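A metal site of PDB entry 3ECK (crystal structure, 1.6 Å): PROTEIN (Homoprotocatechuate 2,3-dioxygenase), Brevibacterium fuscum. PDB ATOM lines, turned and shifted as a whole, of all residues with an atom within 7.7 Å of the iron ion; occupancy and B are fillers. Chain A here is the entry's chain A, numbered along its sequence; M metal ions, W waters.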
ATOM      1  N   ASP A 154      14.883 -33.413   8.504  1.00  0.00           N
ATOM      2  CA  ASP A 154      14.396 -32.671   7.363  1.00  0.00           C
ATOM      3  C   ASP A 154      15.439 -31.848   6.623  1.00  0.00           C
ATOM      4  O   ASP A 154      15.479 -31.901   5.391  1.00  0.00           O
ATOM      5  CB  ASP A 154      13.184 -31.789   7.675  1.00  0.00           C
ATOM      6  CG  ASP A 154      12.567 -31.217   6.411  1.00  0.00           C
ATOM      7  OD1 ASP A 154      11.839 -31.962   5.715  1.00  0.00           O
ATOM      8  OD2 ASP A 154      12.868 -30.047   6.067  1.00  0.00           O
ATOM      9  N   HIS A 155      16.240 -31.088   7.365  1.00  0.00           N
ATOM     10  CA  HIS A 155      17.230 -30.214   6.710  1.00  0.00           C
ATOM     11  C   HIS A 155      18.312 -29.653   7.629  1.00  0.00           C
ATOM     12  O   HIS A 155      18.226 -29.715   8.852  1.00  0.00           O
ATOM     13  CB  HIS A 155      16.517 -29.042   5.999  1.00  0.00           C
ATOM     14  CG  HIS A 155      15.831 -28.098   6.929  1.00  0.00           C
ATOM     15  ND1 HIS A 155      14.478 -28.171   7.211  1.00  0.00           N
ATOM     16  CD2 HIS A 155      16.290 -27.010   7.604  1.00  0.00           C
ATOM     17  CE1 HIS A 155      14.142 -27.177   8.020  1.00  0.00           C
ATOM     18  NE2 HIS A 155      15.224 -26.462   8.285  1.00  0.00           N
ATOM     19  N   PHE A 156      19.326 -29.075   6.983  1.00  0.00           N
ATOM     20  CA  PHE A 156      20.311 -28.264   7.653  1.00  0.00           C
ATOM     21  C   PHE A 156      20.088 -26.796   7.261  1.00  0.00           C
ATOM     22  O   PHE A 156      19.479 -26.495   6.242  1.00  0.00           O
ATOM     23  CB  PHE A 156      21.722 -28.649   7.159  1.00  0.00           C
ATOM     24  CG  PHE A 156      22.044 -30.127   7.263  1.00  0.00           C
ATOM     25  CD1 PHE A 156      21.965 -30.803   8.486  1.00  0.00           C
ATOM     26  CD2 PHE A 156      22.459 -30.834   6.135  1.00  0.00           C
ATOM     27  CE1 PHE A 156      22.280 -32.181   8.560  1.00  0.00           C
ATOM     28  CE2 PHE A 156      22.804 -32.208   6.218  1.00  0.00           C
ATOM     29  CZ  PHE A 156      22.701 -32.870   7.416  1.00  0.00           C
ATOM     30  N   ASN A 157      20.618 -25.896   8.071  1.00  0.00           N
ATOM     31  CA  ASN A 157      20.647 -24.488   7.687  1.00  0.00           C
ATOM     32  C   ASN A 157      21.999 -23.888   8.046  1.00  0.00           C
ATOM     33  O   ASN A 157      22.416 -23.942   9.214  1.00  0.00           O
ATOM     34  CB  ASN A 157      19.481 -23.740   8.343  1.00  0.00           C
ATOM     35  CG  ASN A 157      19.321 -22.338   7.807  1.00  0.00           C
ATOM     36  OD1 ASN A 157      20.275 -21.561   7.849  1.00  0.00           O
ATOM     37  ND2 ASN A 157      18.143 -22.013   7.285  1.00  0.00           N
ATOM     38  N   TRP A 192      16.796 -21.131   0.016  1.00  0.00           N
ATOM     39  CA  TRP A 192      16.428 -22.515   0.406  1.00  0.00           C
ATOM     40  C   TRP A 192      16.573 -23.423  -0.809  1.00  0.00           C
ATOM     41  O   TRP A 192      16.143 -23.069  -1.892  1.00  0.00           O
ATOM     42  CB  TRP A 192      14.963 -22.531   0.873  1.00  0.00           C
ATOM     43  CG  TRP A 192      14.725 -21.976   2.244  1.00  0.00           C
ATOM     44  CD1 TRP A 192      14.476 -22.702   3.374  1.00  0.00           C
ATOM     45  CD2 TRP A 192      14.725 -20.596   2.637  1.00  0.00           C
ATOM     46  NE1 TRP A 192      14.304 -21.847   4.461  1.00  0.00           N
ATOM     47  CE2 TRP A 192      14.452 -20.552   4.031  1.00  0.00           C
ATOM     48  CE3 TRP A 192      14.918 -19.380   1.958  1.00  0.00           C
ATOM     49  CZ2 TRP A 192      14.366 -19.358   4.758  1.00  0.00           C
ATOM     50  CZ3 TRP A 192      14.842 -18.181   2.687  1.00  0.00           C
ATOM     51  CH2 TRP A 192      14.570 -18.181   4.064  1.00  0.00           C
ATOM     52  N   HIS A 200      13.429 -27.881   1.317  1.00  0.00           N
ATOM     53  CA  HIS A 200      14.899 -27.884   1.395  1.00  0.00           C
ATOM     54  C   HIS A 200      15.545 -29.084   2.056  1.00  0.00           C
ATOM     55  O   HIS A 200      14.939 -29.776   2.884  1.00  0.00           O
ATOM     56  CB  HIS A 200      15.482 -26.581   1.967  1.00  0.00           C
ATOM     57  CG  HIS A 200      15.015 -26.213   3.343  1.00  0.00           C
ATOM     58  ND1 HIS A 200      13.705 -26.314   3.745  1.00  0.00           N
ATOM     59  CD2 HIS A 200      15.688 -25.644   4.371  1.00  0.00           C
ATOM     60  CE1 HIS A 200      13.584 -25.849   4.979  1.00  0.00           C
ATOM     61  NE2 HIS A 200      14.775 -25.428   5.378  1.00  0.00           N
ATOM     62  N   ALA A 203      19.969 -24.883   3.459  1.00  0.00           N
ATOM     63  CA  ALA A 203      19.567 -23.507   3.215  1.00  0.00           C
ATOM     64  C   ALA A 203      20.749 -22.631   3.606  1.00  0.00           C
ATOM     65  O   ALA A 203      21.575 -23.029   4.406  1.00  0.00           O
ATOM     66  CB  ALA A 203      18.371 -23.143   4.065  1.00  0.00           C
ATOM     67  N   THR A 205      21.664 -18.904   5.201  1.00  0.00           N
ATOM     68  CA  THR A 205      21.246 -17.698   5.930  1.00  0.00           C
ATOM     69  C   THR A 205      22.428 -16.730   5.909  1.00  0.00           C
ATOM     70  O   THR A 205      23.552 -17.086   6.273  1.00  0.00           O
ATOM     71  CB  THR A 205      20.839 -18.051   7.402  1.00  0.00           C
ATOM     72  OG1 THR A 205      19.751 -18.989   7.392  1.00  0.00           O
ATOM     73  CG2 THR A 205      20.427 -16.782   8.177  1.00  0.00           C
ATOM     74  N   HIS A 213      23.549 -22.864  11.392  1.00  0.00           N
ATOM     75  CA  HIS A 213      22.414 -22.211  12.006  1.00  0.00           C
ATOM     76  C   HIS A 213      21.578 -23.214  12.805  1.00  0.00           C
ATOM     77  O   HIS A 213      21.334 -22.989  13.982  1.00  0.00           O
ATOM     78  CB  HIS A 213      21.543 -21.440  11.021  1.00  0.00           C
ATOM     79  CG  HIS A 213      20.661 -20.446  11.706  1.00  0.00           C
ATOM     80  ND1 HIS A 213      19.466 -20.808  12.300  1.00  0.00           N
ATOM     81  CD2 HIS A 213      20.831 -19.126  11.960  1.00  0.00           C
ATOM     82  CE1 HIS A 213      18.925 -19.744  12.863  1.00  0.00           C
ATOM     83  NE2 HIS A 213      19.721 -18.712  12.664  1.00  0.00           N
ATOM     84  N   HIS A 214      21.157 -24.294  12.142  1.00  0.00           N
ATOM     85  CA  HIS A 214      20.357 -25.345  12.826  1.00  0.00           C
ATOM     86  C   HIS A 214      20.281 -26.649  12.043  1.00  0.00           C
ATOM     87  O   HIS A 214      20.627 -26.703  10.853  1.00  0.00           O
ATOM     88  CB  HIS A 214      18.931 -24.834  13.163  1.00  0.00           C
ATOM     89  CG  HIS A 214      18.121 -24.411  11.972  1.00  0.00           C
ATOM     90  ND1 HIS A 214      18.104 -23.109  11.508  1.00  0.00           N
ATOM     91  CD2 HIS A 214      17.254 -25.103  11.177  1.00  0.00           C
ATOM     92  CE1 HIS A 214      17.282 -23.021  10.476  1.00  0.00           C
ATOM     93  NE2 HIS A 214      16.761 -24.204  10.248  1.00  0.00           N
ATOM     94  N   VAL A 215      19.830 -27.705  12.730  1.00  0.00           N
ATOM     95  CA  VAL A 215      19.431 -28.962  12.144  1.00  0.00           C
ATOM     96  C   VAL A 215      17.924 -29.047  12.439  1.00  0.00           C
ATOM     97  O   VAL A 215      17.510 -28.700  13.558  1.00  0.00           O
ATOM     98  CB  VAL A 215      20.157 -30.158  12.847  1.00  0.00           C
ATOM     99  CG1 VAL A 215      19.719 -31.487  12.285  1.00  0.00           C
ATOM    100  CG2 VAL A 215      21.681 -30.009  12.705  1.00  0.00           C
ATOM    101  N   ALA A 216      17.135 -29.482  11.450  1.00  0.00           N
ATOM    102  CA  ALA A 216      15.671 -29.558  11.622  1.00  0.00           C
ATOM    103  C   ALA A 216      15.183 -30.997  11.539  1.00  0.00           C
ATOM    104  O   ALA A 216      15.589 -31.741  10.638  1.00  0.00           O
ATOM    105  CB  ALA A 216      14.968 -28.724  10.554  1.00  0.00           C
ATOM    106  N   HIS A 248       5.789 -20.578   9.304  1.00  0.00           N
ATOM    107  CA  HIS A 248       6.737 -19.909   8.403  1.00  0.00           C
ATOM    108  C   HIS A 248       6.016 -19.291   7.206  1.00  0.00           C
ATOM    109  O   HIS A 248       5.051 -19.874   6.685  1.00  0.00           O
ATOM    110  CB  HIS A 248       7.776 -20.898   7.870  1.00  0.00           C
ATOM    111  CG  HIS A 248       8.914 -21.209   8.804  1.00  0.00           C
ATOM    112  ND1 HIS A 248       9.620 -20.242   9.486  1.00  0.00           N
ATOM    113  CD2 HIS A 248       9.481 -22.398   9.133  1.00  0.00           C
ATOM    114  CE1 HIS A 248      10.559 -20.820  10.206  1.00  0.00           C
ATOM    115  NE2 HIS A 248      10.523 -22.132   9.990  1.00  0.00           N
ATOM    116  N   SER A 251       8.498 -21.477   3.020  1.00  0.00           N
ATOM    117  CA  SER A 251       8.345 -22.924   3.279  1.00  0.00           C
ATOM    118  C   SER A 251       6.911 -23.320   3.700  1.00  0.00           C
ATOM    119  O   SER A 251       6.529 -24.457   3.509  1.00  0.00           O
ATOM    120  CB  SER A 251       9.378 -23.515   4.269  1.00  0.00           C
ATOM    121  OG  SER A 251       8.984 -23.300   5.641  1.00  0.00           O
ATOM    122  N   TYR A 255       6.567 -24.501  12.804  1.00  0.00           N
ATOM    123  CA  TYR A 255       7.958 -24.563  13.275  1.00  0.00           C
ATOM    124  C   TYR A 255       8.146 -24.219  14.746  1.00  0.00           C
ATOM    125  O   TYR A 255       7.282 -23.547  15.368  1.00  0.00           O
ATOM    126  CB  TYR A 255       8.853 -23.637  12.425  1.00  0.00           C
ATOM    127  CG  TYR A 255       8.638 -22.190  12.730  1.00  0.00           C
ATOM    128  CD1 TYR A 255       7.760 -21.411  11.968  1.00  0.00           C
ATOM    129  CD2 TYR A 255       9.330 -21.578  13.783  1.00  0.00           C
ATOM    130  CE1 TYR A 255       7.566 -20.049  12.256  1.00  0.00           C
ATOM    131  CE2 TYR A 255       9.147 -20.225  14.091  1.00  0.00           C
ATOM    132  CZ  TYR A 255       8.270 -19.465  13.314  1.00  0.00           C
ATOM    133  OH  TYR A 255       8.130 -18.132  13.624  1.00  0.00           O
ATOM    134  N   LEU A 256       9.316 -24.597  15.262  1.00  0.00           N
ATOM    135  CA  LEU A 256       9.760 -24.227  16.586  1.00  0.00           C
ATOM    136  C   LEU A 256      11.287 -24.278  16.603  1.00  0.00           C
ATOM    137  O   LEU A 256      11.851 -25.174  15.983  1.00  0.00           O
ATOM    138  CB  LEU A 256       9.210 -25.242  17.595  1.00  0.00           C
ATOM    139  CG  LEU A 256       9.691 -25.097  19.031  1.00  0.00           C
ATOM    140  CD1 LEU A 256       9.138 -23.821  19.713  1.00  0.00           C
ATOM    141  CD2 LEU A 256       9.300 -26.356  19.831  1.00  0.00           C
ATOM    142  N   TYR A 257      11.945 -23.329  17.284  1.00  0.00           N
ATOM    143  CA  TYR A 257      13.389 -23.393  17.513  1.00  0.00           C
ATOM    144  C   TYR A 257      13.716 -23.492  18.994  1.00  0.00           C
ATOM    145  O   TYR A 257      13.260 -22.672  19.800  1.00  0.00           O
ATOM    146  CB  TYR A 257      14.119 -22.181  16.911  1.00  0.00           C
ATOM    147  CG  TYR A 257      13.896 -21.994  15.437  1.00  0.00           C
ATOM    148  CD1 TYR A 257      14.724 -22.611  14.494  1.00  0.00           C
ATOM    149  CD2 TYR A 257      12.852 -21.188  14.976  1.00  0.00           C
ATOM    150  CE1 TYR A 257      14.510 -22.434  13.108  1.00  0.00           C
ATOM    151  CE2 TYR A 257      12.601 -21.008  13.597  1.00  0.00           C
ATOM    152  CZ  TYR A 257      13.437 -21.625  12.669  1.00  0.00           C
ATOM    153  OH  TYR A 257      13.190 -21.424  11.329  1.00  0.00           O
ATOM    154  N   GLU A 267      15.544 -27.097  15.030  1.00  0.00           N
ATOM    155  CA  GLU A 267      14.208 -26.712  14.594  1.00  0.00           C
ATOM    156  C   GLU A 267      13.316 -27.944  14.524  1.00  0.00           C
ATOM    157  O   GLU A 267      13.752 -29.007  14.078  1.00  0.00           O
ATOM    158  CB  GLU A 267      14.240 -26.055  13.211  1.00  0.00           C
ATOM    159  CG  GLU A 267      12.866 -25.451  12.790  1.00  0.00           C
ATOM    160  CD  GLU A 267      12.883 -24.895  11.382  1.00  0.00           C
ATOM    161  OE1 GLU A 267      13.964 -24.971  10.753  1.00  0.00           O
ATOM    162  OE2 GLU A 267      11.826 -24.405  10.936  1.00  0.00           O
ATOM    163  N   ILE A 268      12.074 -27.781  14.976  1.00  0.00           N
ATOM    164  CA  ILE A 268      11.052 -28.775  14.728  1.00  0.00           C
ATOM    165  C   ILE A 268      10.112 -28.185  13.672  1.00  0.00           C
ATOM    166  O   ILE A 268       9.759 -27.001  13.727  1.00  0.00           O
ATOM    167  CB  ILE A 268      10.281 -29.136  16.025  1.00  0.00           C
ATOM    168  CG1 ILE A 268      11.220 -29.153  17.248  1.00  0.00           C
ATOM    169  CG2 ILE A 268       9.619 -30.469  15.833  1.00  0.00           C
ATOM    170  CD1 ILE A 268      12.273 -30.231  17.211  1.00  0.00           C
ATOM    171  N   TYR A 269       9.710 -29.001  12.709  1.00  0.00           N
ATOM    172  CA  TYR A 269       9.211 -28.527  11.427  1.00  0.00           C
ATOM    173  C   TYR A 269       8.143 -29.513  10.952  1.00  0.00           C
ATOM    174  O   TYR A 269       8.305 -30.740  11.101  1.00  0.00           O
ATOM    175  CB  TYR A 269      10.427 -28.537  10.494  1.00  0.00           C
ATOM    176  CG  TYR A 269      10.310 -28.053   9.085  1.00  0.00           C
ATOM    177  CD1 TYR A 269      10.610 -26.721   8.757  1.00  0.00           C
ATOM    178  CD2 TYR A 269      10.007 -28.948   8.043  1.00  0.00           C
ATOM    179  CE1 TYR A 269      10.569 -26.294   7.434  1.00  0.00           C
ATOM    180  CE2 TYR A 269       9.954 -28.517   6.713  1.00  0.00           C
ATOM    181  CZ  TYR A 269      10.243 -27.179   6.425  1.00  0.00           C
ATOM    182  OH  TYR A 269      10.219 -26.725   5.121  1.00  0.00           O
ATOM    183  N   ARG A 293       8.962 -14.594   7.537  1.00  0.00           N
ATOM    184  CA  ARG A 293       9.616 -15.576   8.426  1.00  0.00           C
ATOM    185  C   ARG A 293       8.616 -16.185   9.386  1.00  0.00           C
ATOM    186  O   ARG A 293       8.575 -17.418   9.548  1.00  0.00           O
ATOM    187  CB  ARG A 293      10.819 -14.974   9.159  1.00  0.00           C
ATOM    188  CG  ARG A 293      12.017 -14.795   8.215  1.00  0.00           C
ATOM    189  CD  ARG A 293      13.339 -14.685   8.946  1.00  0.00           C
ATOM    190  NE  ARG A 293      14.498 -14.584   8.039  1.00  0.00           N
ATOM    191  CZ  ARG A 293      15.143 -15.614   7.492  1.00  0.00           C
ATOM    192  NH1 ARG A 293      14.775 -16.866   7.750  1.00  0.00           N
ATOM    193  NH2 ARG A 293      16.201 -15.396   6.694  1.00  0.00           N
ATOM    194  N   TRP A 304      18.222 -15.193  16.962  1.00  0.00           N
ATOM    195  CA  TRP A 304      18.047 -16.037  15.792  1.00  0.00           C
ATOM    196  C   TRP A 304      18.954 -15.552  14.637  1.00  0.00           C
ATOM    197  O   TRP A 304      19.478 -16.354  13.840  1.00  0.00           O
ATOM    198  CB  TRP A 304      16.554 -16.116  15.370  1.00  0.00           C
ATOM    199  CG  TRP A 304      16.243 -17.289  14.501  1.00  0.00           C
ATOM    200  CD1 TRP A 304      15.823 -18.525  14.915  1.00  0.00           C
ATOM    201  CD2 TRP A 304      16.308 -17.348  13.064  1.00  0.00           C
ATOM    202  NE1 TRP A 304      15.641 -19.348  13.836  1.00  0.00           N
ATOM    203  CE2 TRP A 304      15.925 -18.660  12.677  1.00  0.00           C
ATOM    204  CE3 TRP A 304      16.678 -16.431  12.057  1.00  0.00           C
ATOM    205  CZ2 TRP A 304      15.899 -19.081  11.356  1.00  0.00           C
ATOM    206  CZ3 TRP A 304      16.655 -16.856  10.726  1.00  0.00           C
ATOM    207  CH2 TRP A 304      16.265 -18.171  10.383  1.00  0.00           C
HETATM  208 FE    FE M   1      14.951 -24.398   9.036  1.00  0.00          FE
HETATM  209  O   HOH W   1      12.908 -24.223   8.209  1.00  0.00           O
HETATM  210  O   HOH W   2      14.623 -22.159   9.391  1.00  0.00           O
HETATM  211  O   HOH W   3      15.933 -23.615   7.248  1.00  0.00           O
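OE2 of Glu 267 lies within hydrogen-bond range of OH of Tyr 257, 3.3 Å away.
OE2 of Glu 267 sits at hydrogen-bond distance from NE2 of His 248 (2.8 Å).
The backbone carbonyl oxygen of Val 215 sits at hydrogen-bond distance from the backbone NH of Glu 267 (2.9 Å).
N of Asn 157 lies within hydrogen-bond range of O of His 214 (2.9 Å).
A ring nitrogen (ND1) of His 214 sits at hydrogen-bond distance from a ring nitrogen (ND1) of His 213, 2.8 Å away.
NE2 of His 200 sits close to ND1 of His 155, at 3.3 Å.
The backbone NH (N) of Ala 216 lies within hydrogen-bond range of the backbone carbonyl oxygen (O) of His 155 (2.8 Å).
OD2 of Asp 154 lies within hydrogen-bond range of ND1 of His 155 (2.7 Å).
Merely in contact with the iron ion: His 200 (3.8 Å).
Four residues have an atom within 4 Å of the iron ion: His 155, His 200, His 214 and Glu 267.
The nearest printed residue that does not touch the iron ion is Tyr 257 (4.1 Å).
The iron ion is bound by the side-chain carboxylate (OE1) of Glu 267 (2.1 Å), water W3 (2.2 Å), a ring nitrogen (NE2) of His 214 (2.2 Å), water W1 (2.2 Å), a ring nitrogen (NE2) of His 155 (2.2 Å) and water W2 (2.3 Å).
Water W3 lies within hydrogen-bond range of the side-chain amide nitrogen of Asn 157 (2.7 Å) and a ring nitrogen (NE2) of His 200 (2.9 Å).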
